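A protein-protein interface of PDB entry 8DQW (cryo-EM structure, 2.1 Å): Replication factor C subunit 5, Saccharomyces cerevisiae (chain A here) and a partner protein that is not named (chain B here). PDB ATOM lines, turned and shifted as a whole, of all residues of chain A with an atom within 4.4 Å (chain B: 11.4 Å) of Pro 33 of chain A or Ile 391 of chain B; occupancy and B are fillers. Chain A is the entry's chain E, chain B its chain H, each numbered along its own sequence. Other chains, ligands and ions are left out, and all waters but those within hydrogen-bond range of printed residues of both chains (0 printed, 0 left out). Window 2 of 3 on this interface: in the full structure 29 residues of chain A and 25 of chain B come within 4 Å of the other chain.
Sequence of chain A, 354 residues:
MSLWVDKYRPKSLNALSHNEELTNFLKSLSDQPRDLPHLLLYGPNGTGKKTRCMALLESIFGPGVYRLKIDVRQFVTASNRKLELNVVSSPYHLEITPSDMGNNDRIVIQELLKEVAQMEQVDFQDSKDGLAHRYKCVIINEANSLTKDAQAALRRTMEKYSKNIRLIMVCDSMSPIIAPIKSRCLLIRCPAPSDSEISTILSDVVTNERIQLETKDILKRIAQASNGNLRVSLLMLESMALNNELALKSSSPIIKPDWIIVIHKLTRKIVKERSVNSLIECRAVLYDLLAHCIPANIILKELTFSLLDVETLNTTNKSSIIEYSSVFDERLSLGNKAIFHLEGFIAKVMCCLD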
ATOM      1  N   LEU A  29      30.179  10.181 -10.593  1.00  0.00           N
ATOM      2  CA  LEU A  29      29.976   8.756 -10.842  1.00  0.00           C
ATOM      3  C   LEU A  29      29.941   7.971  -9.536  1.00  0.00           C
ATOM      4  O   LEU A  29      29.137   7.046  -9.382  1.00  0.00           O
ATOM      5  CB  LEU A  29      31.077   8.219 -11.757  1.00  0.00           C
ATOM      6  CG  LEU A  29      30.885   8.423 -13.264  1.00  0.00           C
ATOM      7  CD1 LEU A  29      32.100   7.914 -14.024  1.00  0.00           C
ATOM      8  CD2 LEU A  29      29.618   7.740 -13.760  1.00  0.00           C
ATOM      9  N   SER A  30      30.806   8.328  -8.585  1.00  0.00           N
ATOM     10  CA  SER A  30      30.886   7.615  -7.315  1.00  0.00           C
ATOM     11  C   SER A  30      29.744   7.945  -6.361  1.00  0.00           C
ATOM     12  O   SER A  30      29.643   7.307  -5.308  1.00  0.00           O
ATOM     13  CB  SER A  30      32.212   7.923  -6.615  1.00  0.00           C
ATOM     14  OG  SER A  30      33.312   7.684  -7.470  1.00  0.00           O
ATOM     15  N   ASP A  31      28.898   8.925  -6.685  1.00  0.00           N
ATOM     16  CA  ASP A  31      27.822   9.298  -5.773  1.00  0.00           C
ATOM     17  C   ASP A  31      26.881   8.126  -5.524  1.00  0.00           C
ATOM     18  O   ASP A  31      26.584   7.785  -4.372  1.00  0.00           O
ATOM     19  CB  ASP A  31      27.055  10.495  -6.335  1.00  0.00           C
ATOM     20  CG  ASP A  31      26.074  11.079  -5.338  1.00  0.00           C
ATOM     21  OD1 ASP A  31      26.407  11.125  -4.134  1.00  0.00           O
ATOM     22  OD2 ASP A  31      24.972  11.491  -5.756  1.00  0.00           O
ATOM     23  N   GLN A  32      26.405   7.491  -6.594  1.00  0.00           N
ATOM     24  CA  GLN A  32      25.505   6.340  -6.513  1.00  0.00           C
ATOM     25  C   GLN A  32      26.076   5.233  -7.388  1.00  0.00           C
ATOM     26  O   GLN A  32      25.611   5.011  -8.513  1.00  0.00           O
ATOM     27  CB  GLN A  32      24.086   6.710  -6.944  1.00  0.00           C
ATOM     28  CG  GLN A  32      23.464   7.852  -6.152  1.00  0.00           C
ATOM     29  CD  GLN A  32      22.891   7.395  -4.825  1.00  0.00           C
ATOM     30  OE1 GLN A  32      23.526   7.536  -3.780  1.00  0.00           O
ATOM     31  NE2 GLN A  32      21.685   6.841  -4.861  1.00  0.00           N
ATOM     32  N   PRO A  33      27.089   4.509  -6.899  1.00  0.00           N
ATOM     33  CA  PRO A  33      27.735   3.481  -7.729  1.00  0.00           C
ATOM     34  C   PRO A  33      26.884   2.235  -7.918  1.00  0.00           C
ATOM     35  O   PRO A  33      27.332   1.250  -8.511  1.00  0.00           O
ATOM     36  CB  PRO A  33      29.011   3.177  -6.936  1.00  0.00           C
ATOM     37  CG  PRO A  33      28.555   3.344  -5.523  1.00  0.00           C
ATOM     38  CD  PRO A  33      27.751   4.617  -5.587  1.00  0.00           C
ATOM     39  N   ARG A  34      25.652   2.275  -7.410  1.00  0.00           N
ATOM     40  CA  ARG A  34      24.770   1.118  -7.491  1.00  0.00           C
ATOM     41  C   ARG A  34      24.470   0.753  -8.942  1.00  0.00           C
ATOM     42  O   ARG A  34      24.433  -0.432  -9.297  1.00  0.00           O
ATOM     43  CB  ARG A  34      23.490   1.415  -6.703  1.00  0.00           C
ATOM     44  CG  ARG A  34      23.583   1.002  -5.234  1.00  0.00           C
ATOM     45  CD  ARG A  34      22.251   0.533  -4.652  1.00  0.00           C
ATOM     46  NE  ARG A  34      22.400  -0.132  -3.360  1.00  0.00           N
ATOM     47  CZ  ARG A  34      22.999   0.381  -2.292  1.00  0.00           C
ATOM     48  NH1 ARG A  34      23.446   1.627  -2.271  1.00  0.00           N
ATOM     49  NH2 ARG A  34      23.140  -0.374  -1.205  1.00  0.00           N
ATOM     50  N   ASP A  35      24.273   1.754  -9.799  1.00  0.00           N
ATOM     51  CA  ASP A  35      23.960   1.548 -11.210  1.00  0.00           C
ATOM     52  C   ASP A  35      25.082   2.053 -12.114  1.00  0.00           C
ATOM     53  O   ASP A  35      24.836   2.629 -13.176  1.00  0.00           O
ATOM     54  CB  ASP A  35      22.641   2.226 -11.571  1.00  0.00           C
ATOM     55  CG  ASP A  35      22.600   3.685 -11.155  1.00  0.00           C
ATOM     56  OD1 ASP A  35      23.660   4.228 -10.780  1.00  0.00           O
ATOM     57  OD2 ASP A  35      21.507   4.284 -11.201  1.00  0.00           O
ATOM     58  N   LEU A  36      26.326   1.837 -11.706  1.00  0.00           N
ATOM     59  CA  LEU A  36      27.476   2.266 -12.490  1.00  0.00           C
ATOM     60  C   LEU A  36      27.545   1.487 -13.802  1.00  0.00           C
ATOM     61  O   LEU A  36      27.583   0.248 -13.770  1.00  0.00           O
ATOM     62  CB  LEU A  36      28.757   2.055 -11.685  1.00  0.00           C
ATOM     63  CG  LEU A  36      30.090   2.369 -12.370  1.00  0.00           C
ATOM     64  CD1 LEU A  36      30.400   3.854 -12.287  1.00  0.00           C
ATOM     65  CD2 LEU A  36      31.207   1.550 -11.742  1.00  0.00           C
ATOM     66  N   ILE A  60      34.504   3.953  -4.243  1.00  0.00           N
ATOM     67  CA  ILE A  60      33.382   3.024  -4.142  1.00  0.00           C
ATOM     68  C   ILE A  60      33.565   2.083  -2.956  1.00  0.00           C
ATOM     69  O   ILE A  60      32.657   1.914  -2.134  1.00  0.00           O
ATOM     70  CB  ILE A  60      33.212   2.240  -5.456  1.00  0.00           C
ATOM     71  CG1 ILE A  60      32.710   3.164  -6.566  1.00  0.00           C
ATOM     72  CG2 ILE A  60      32.244   1.080  -5.262  1.00  0.00           C
ATOM     73  CD1 ILE A  60      33.238   2.809  -7.935  1.00  0.00           C
ATOM     74  N   PHE A  61      34.738   1.457  -2.847  1.00  0.00           N
ATOM     75  CA  PHE A  61      34.968   0.403  -1.862  1.00  0.00           C
ATOM     76  C   PHE A  61      35.750   0.897  -0.647  1.00  0.00           C
ATOM     77  O   PHE A  61      35.265   0.802   0.484  1.00  0.00           O
ATOM     78  CB  PHE A  61      35.700  -0.769  -2.528  1.00  0.00           C
ATOM     79  CG  PHE A  61      34.895  -1.457  -3.594  1.00  0.00           C
ATOM     80  CD1 PHE A  61      33.899  -2.360  -3.254  1.00  0.00           C
ATOM     81  CD2 PHE A  61      35.127  -1.197  -4.934  1.00  0.00           C
ATOM     82  CE1 PHE A  61      33.156  -2.994  -4.231  1.00  0.00           C
ATOM     83  CE2 PHE A  61      34.386  -1.826  -5.917  1.00  0.00           C
ATOM     84  CZ  PHE A  61      33.399  -2.727  -5.564  1.00  0.00           C
ATOM     85  N   HIS A 133      24.527  -9.167  -1.937  1.00  0.00           N
ATOM     86  CA  HIS A 133      25.135  -9.308  -3.252  1.00  0.00           C
ATOM     87  C   HIS A 133      25.915  -8.047  -3.600  1.00  0.00           C
ATOM     88  O   HIS A 133      25.513  -6.937  -3.240  1.00  0.00           O
ATOM     89  CB  HIS A 133      24.068  -9.573  -4.317  1.00  0.00           C
ATOM     90  CG  HIS A 133      24.596  -9.564  -5.718  1.00  0.00           C
ATOM     91  ND1 HIS A 133      24.311  -8.558  -6.614  1.00  0.00           N
ATOM     92  CD2 HIS A 133      25.397 -10.437  -6.372  1.00  0.00           C
ATOM     93  CE1 HIS A 133      24.909  -8.814  -7.765  1.00  0.00           C
ATOM     94  NE2 HIS A 133      25.576  -9.948  -7.643  1.00  0.00           N
ATOM     95  N   ARG A 134      27.033  -8.228  -4.299  1.00  0.00           N
ATOM     96  CA  ARG A 134      27.889  -7.124  -4.715  1.00  0.00           C
ATOM     97  C   ARG A 134      28.505  -7.464  -6.062  1.00  0.00           C
ATOM     98  O   ARG A 134      29.040  -8.562  -6.238  1.00  0.00           O
ATOM     99  CB  ARG A 134      28.990  -6.865  -3.682  1.00  0.00           C
ATOM    100  CG  ARG A 134      28.608  -5.869  -2.597  1.00  0.00           C
ATOM    101  CD  ARG A 134      29.711  -5.702  -1.555  1.00  0.00           C
ATOM    102  NE  ARG A 134      30.693  -6.782  -1.597  1.00  0.00           N
ATOM    103  CZ  ARG A 134      30.709  -7.829  -0.781  1.00  0.00           C
ATOM    104  NH1 ARG A 134      29.797  -7.987   0.166  1.00  0.00           N
ATOM    105  NH2 ARG A 134      31.662  -8.745  -0.922  1.00  0.00           N
ATOM    106  N   TYR A 135      28.434  -6.530  -7.007  1.00  0.00           N
ATOM    107  CA  TYR A 135      29.030  -6.773  -8.312  1.00  0.00           C
ATOM    108  C   TYR A 135      30.550  -6.695  -8.224  1.00  0.00           C
ATOM    109  O   TYR A 135      31.113  -5.968  -7.403  1.00  0.00           O
ATOM    110  CB  TYR A 135      28.493  -5.784  -9.353  1.00  0.00           C
ATOM    111  CG  TYR A 135      28.851  -4.322  -9.147  1.00  0.00           C
ATOM    112  CD1 TYR A 135      30.160  -3.871  -9.286  1.00  0.00           C
ATOM    113  CD2 TYR A 135      27.869  -3.387  -8.845  1.00  0.00           C
ATOM    114  CE1 TYR A 135      30.481  -2.539  -9.108  1.00  0.00           C
ATOM    115  CE2 TYR A 135      28.181  -2.052  -8.667  1.00  0.00           C
ATOM    116  CZ  TYR A 135      29.489  -1.633  -8.801  1.00  0.00           C
ATOM    117  OH  TYR A 135      29.803  -0.306  -8.626  1.00  0.00           O
ATOM    118  N   THR B  59      36.871 -14.761  -1.484  1.00  0.00           N
ATOM    119  CA  THR B  59      35.463 -14.533  -1.796  1.00  0.00           C
ATOM    120  C   THR B  59      35.281 -14.106  -3.248  1.00  0.00           C
ATOM    121  O   THR B  59      34.393 -14.606  -3.947  1.00  0.00           O
ATOM    122  CB  THR B  59      34.884 -13.479  -0.851  1.00  0.00           C
ATOM    123  OG1 THR B  59      35.058 -13.902   0.506  1.00  0.00           O
ATOM    124  CG2 THR B  59      33.403 -13.263  -1.129  1.00  0.00           C
ATOM    125  N   ILE B  60      36.119 -13.183  -3.724  1.00  0.00           N
ATOM    126  CA  ILE B  60      35.927 -12.650  -5.068  1.00  0.00           C
ATOM    127  C   ILE B  60      36.481 -13.594  -6.131  1.00  0.00           C
ATOM    128  O   ILE B  60      35.999 -13.599  -7.269  1.00  0.00           O
ATOM    129  CB  ILE B  60      36.559 -11.253  -5.185  1.00  0.00           C
ATOM    130  CG1 ILE B  60      36.146 -10.597  -6.505  1.00  0.00           C
ATOM    131  CG2 ILE B  60      38.077 -11.336  -5.088  1.00  0.00           C
ATOM    132  CD1 ILE B  60      36.370  -9.104  -6.543  1.00  0.00           C
ATOM    133  N   ASP B 390      27.366   1.886   0.317  1.00  0.00           N
ATOM    134  CA  ASP B 390      28.063   0.846  -0.432  1.00  0.00           C
ATOM    135  C   ASP B 390      27.178   0.319  -1.561  1.00  0.00           C
ATOM    136  O   ASP B 390      26.085   0.837  -1.794  1.00  0.00           O
ATOM    137  CB  ASP B 390      28.486  -0.290   0.502  1.00  0.00           C
ATOM    138  CG  ASP B 390      27.427  -0.623   1.533  1.00  0.00           C
ATOM    139  OD1 ASP B 390      26.945   0.306   2.215  1.00  0.00           O
ATOM    140  OD2 ASP B 390      27.078  -1.814   1.666  1.00  0.00           O
ATOM    141  N   ILE B 391      27.656  -0.710  -2.260  1.00  0.00           N
ATOM    142  CA  ILE B 391      26.952  -1.268  -3.409  1.00  0.00           C
ATOM    143  C   ILE B 391      26.240  -2.573  -3.068  1.00  0.00           C
ATOM    144  O   ILE B 391      25.783  -3.279  -3.973  1.00  0.00           O
ATOM    145  CB  ILE B 391      27.912  -1.469  -4.593  1.00  0.00           C
ATOM    146  CG1 ILE B 391      29.110  -2.326  -4.172  1.00  0.00           C
ATOM    147  CG2 ILE B 391      28.390  -0.128  -5.120  1.00  0.00           C
ATOM    148  CD1 ILE B 391      29.449  -3.422  -5.157  1.00  0.00           C
ATOM    149  N   SER B 392      26.130  -2.911  -1.786  1.00  0.00           N
ATOM    150  CA  SER B 392      25.513  -4.171  -1.398  1.00  0.00           C
ATOM    151  C   SER B 392      24.002  -4.120  -1.588  1.00  0.00           C
ATOM    152  O   SER B 392      23.358  -3.101  -1.321  1.00  0.00           O
ATOM    153  CB  SER B 392      25.843  -4.500   0.057  1.00  0.00           C
ATOM    154  OG  SER B 392      27.025  -5.275   0.149  1.00  0.00           O
ATOM    155  N   VAL B 393      23.438  -5.233  -2.059  1.00  0.00           N
ATOM    156  CA  VAL B 393      21.996  -5.395  -2.192  1.00  0.00           C
ATOM    157  C   VAL B 393      21.627  -6.806  -1.757  1.00  0.00           C
ATOM    158  O   VAL B 393      22.468  -7.706  -1.704  1.00  0.00           O
ATOM    159  CB  VAL B 393      21.502  -5.141  -3.633  1.00  0.00           C
ATOM    160  CG1 VAL B 393      21.416  -3.647  -3.911  1.00  0.00           C
ATOM    161  CG2 VAL B 393      22.412  -5.837  -4.636  1.00  0.00           C
ATOM    162  N   MET B 394      20.349  -6.990  -1.443  1.00  0.00           N
ATOM    163  CA  MET B 394      19.858  -8.304  -1.053  1.00  0.00           C
ATOM    164  C   MET B 394      19.795  -9.228  -2.263  1.00  0.00           C
ATOM    165  O   MET B 394      19.437  -8.810  -3.366  1.00  0.00           O
ATOM    166  CB  MET B 394      18.474  -8.183  -0.413  1.00  0.00           C
ATOM    167  CG  MET B 394      18.455  -7.484   0.944  1.00  0.00           C
ATOM    168  SD  MET B 394      19.721  -8.058   2.094  1.00  0.00           S
ATOM    169  CE  MET B 394      19.335  -9.806   2.183  1.00  0.00           C
ATOM    170  N   VAL B 395      20.148 -10.496  -2.047  1.00  0.00           N
ATOM    171  CA  VAL B 395      20.105 -11.474  -3.127  1.00  0.00           C
ATOM    172  C   VAL B 395      18.658 -11.712  -3.545  1.00  0.00           C
ATOM    173  O   VAL B 395      17.722 -11.589  -2.745  1.00  0.00           O
ATOM    174  CB  VAL B 395      20.776 -12.792  -2.700  1.00  0.00           C
ATOM    175  CG1 VAL B 395      22.213 -12.545  -2.270  1.00  0.00           C
ATOM    176  CG2 VAL B 395      19.983 -13.462  -1.583  1.00  0.00           C
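Hydrophobic or aromatic side chains of chain B within 4 Å of the printed part of chain A: Ile 391 and Val 393. Among the printed residues, 11 pairs touch across the chains.
Ile 391 of chain B touches just these residues of chain A: Pro 33, Phe 61, His 133, Arg 134 and Tyr 135. No residue of chain B comes within 4 Å of Ser 30 of chain A. No residue of chain B comes within 4 Å of Gln 32 of chain A. Of chain B, only Asp 390 (2.8 Å), Ser 392 (2.7 Å) and Val 393 (3.7 Å) come within 4 Å of Arg 34 of chain A. No residue of chain B comes within 4 Å of Asp 35 of chain A. No residue of chain B comes within 4 Å of Leu 36 of chain A. No residue of chain B comes within 4 Å of Ile 60 of chain A. Of chain B, only Ile 391 and Ser 392 come within 4 Å of Arg 134 of chain A. Of chain B, only Ile 391 (3.8 Å) comes within 4 Å of Tyr 135 of chain A. Printed residues of chain B within 4 Å of Phe 61 of chain A: Ile 391. Printed residues of chain A within 4 Å of Ser 392 of chain B: Arg 34, His 133 and Arg 134. Printed residues of chain A within 4 Å of Asp 390 of chain B: Arg 34. Ile 60 of chain B touches none of the printed residues of chain A. Thr 59 of chain B touches none of the printed residues of chain A. The nearest printed residue of chain B that does not touch His 133 of chain A is Val 395 of chain B (4.1 Å).
The guanidinium group (NH1) of Arg 34 of chain A lies within hydrogen-bond range of the backbone carbonyl oxygen (O) of Asp 390 of chain B (2.8 Å). The guanidinium group (NH2) of Arg 34 of chain A lies within hydrogen-bond range of the backbone carbonyl oxygen (O) of Ser 392 of chain B, at 2.7 Å. N of His 133 of chain A lies within hydrogen-bond range of O of Val 393 of chain B (2.5 Å).
CG2 of Ile 391 of chain B touches CG of Pro 33 of chain A (3.5 Å). NE of Arg 34 of chain A touches CG1 of Val 393 of chain B, 3.7 Å away. CE1 of Phe 61 of chain A touches CD1 of Ile 391 of chain B (3.8 Å). O of His 133 of chain A touches O of Ile 391 of chain B, 3.7 Å away. CA of Ser 392 of chain B touches O of His 133 of chain A, at 3.3 Å. CG of Arg 134 of chain A touches CD1 of Ile 391 of chain B (3.6 Å). Ser 392 of chain B touches Arg 134 of chain A. Ile 391 of chain B touches Tyr 135 of chain A (CD1 to N, 3.8 Å).
The side-chain hydroxyl of Tyr 135 of chain A sits at hydrogen-bond distance from the backbone carbonyl oxygen of Pro 33 of chain A, at 2.9 Å.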
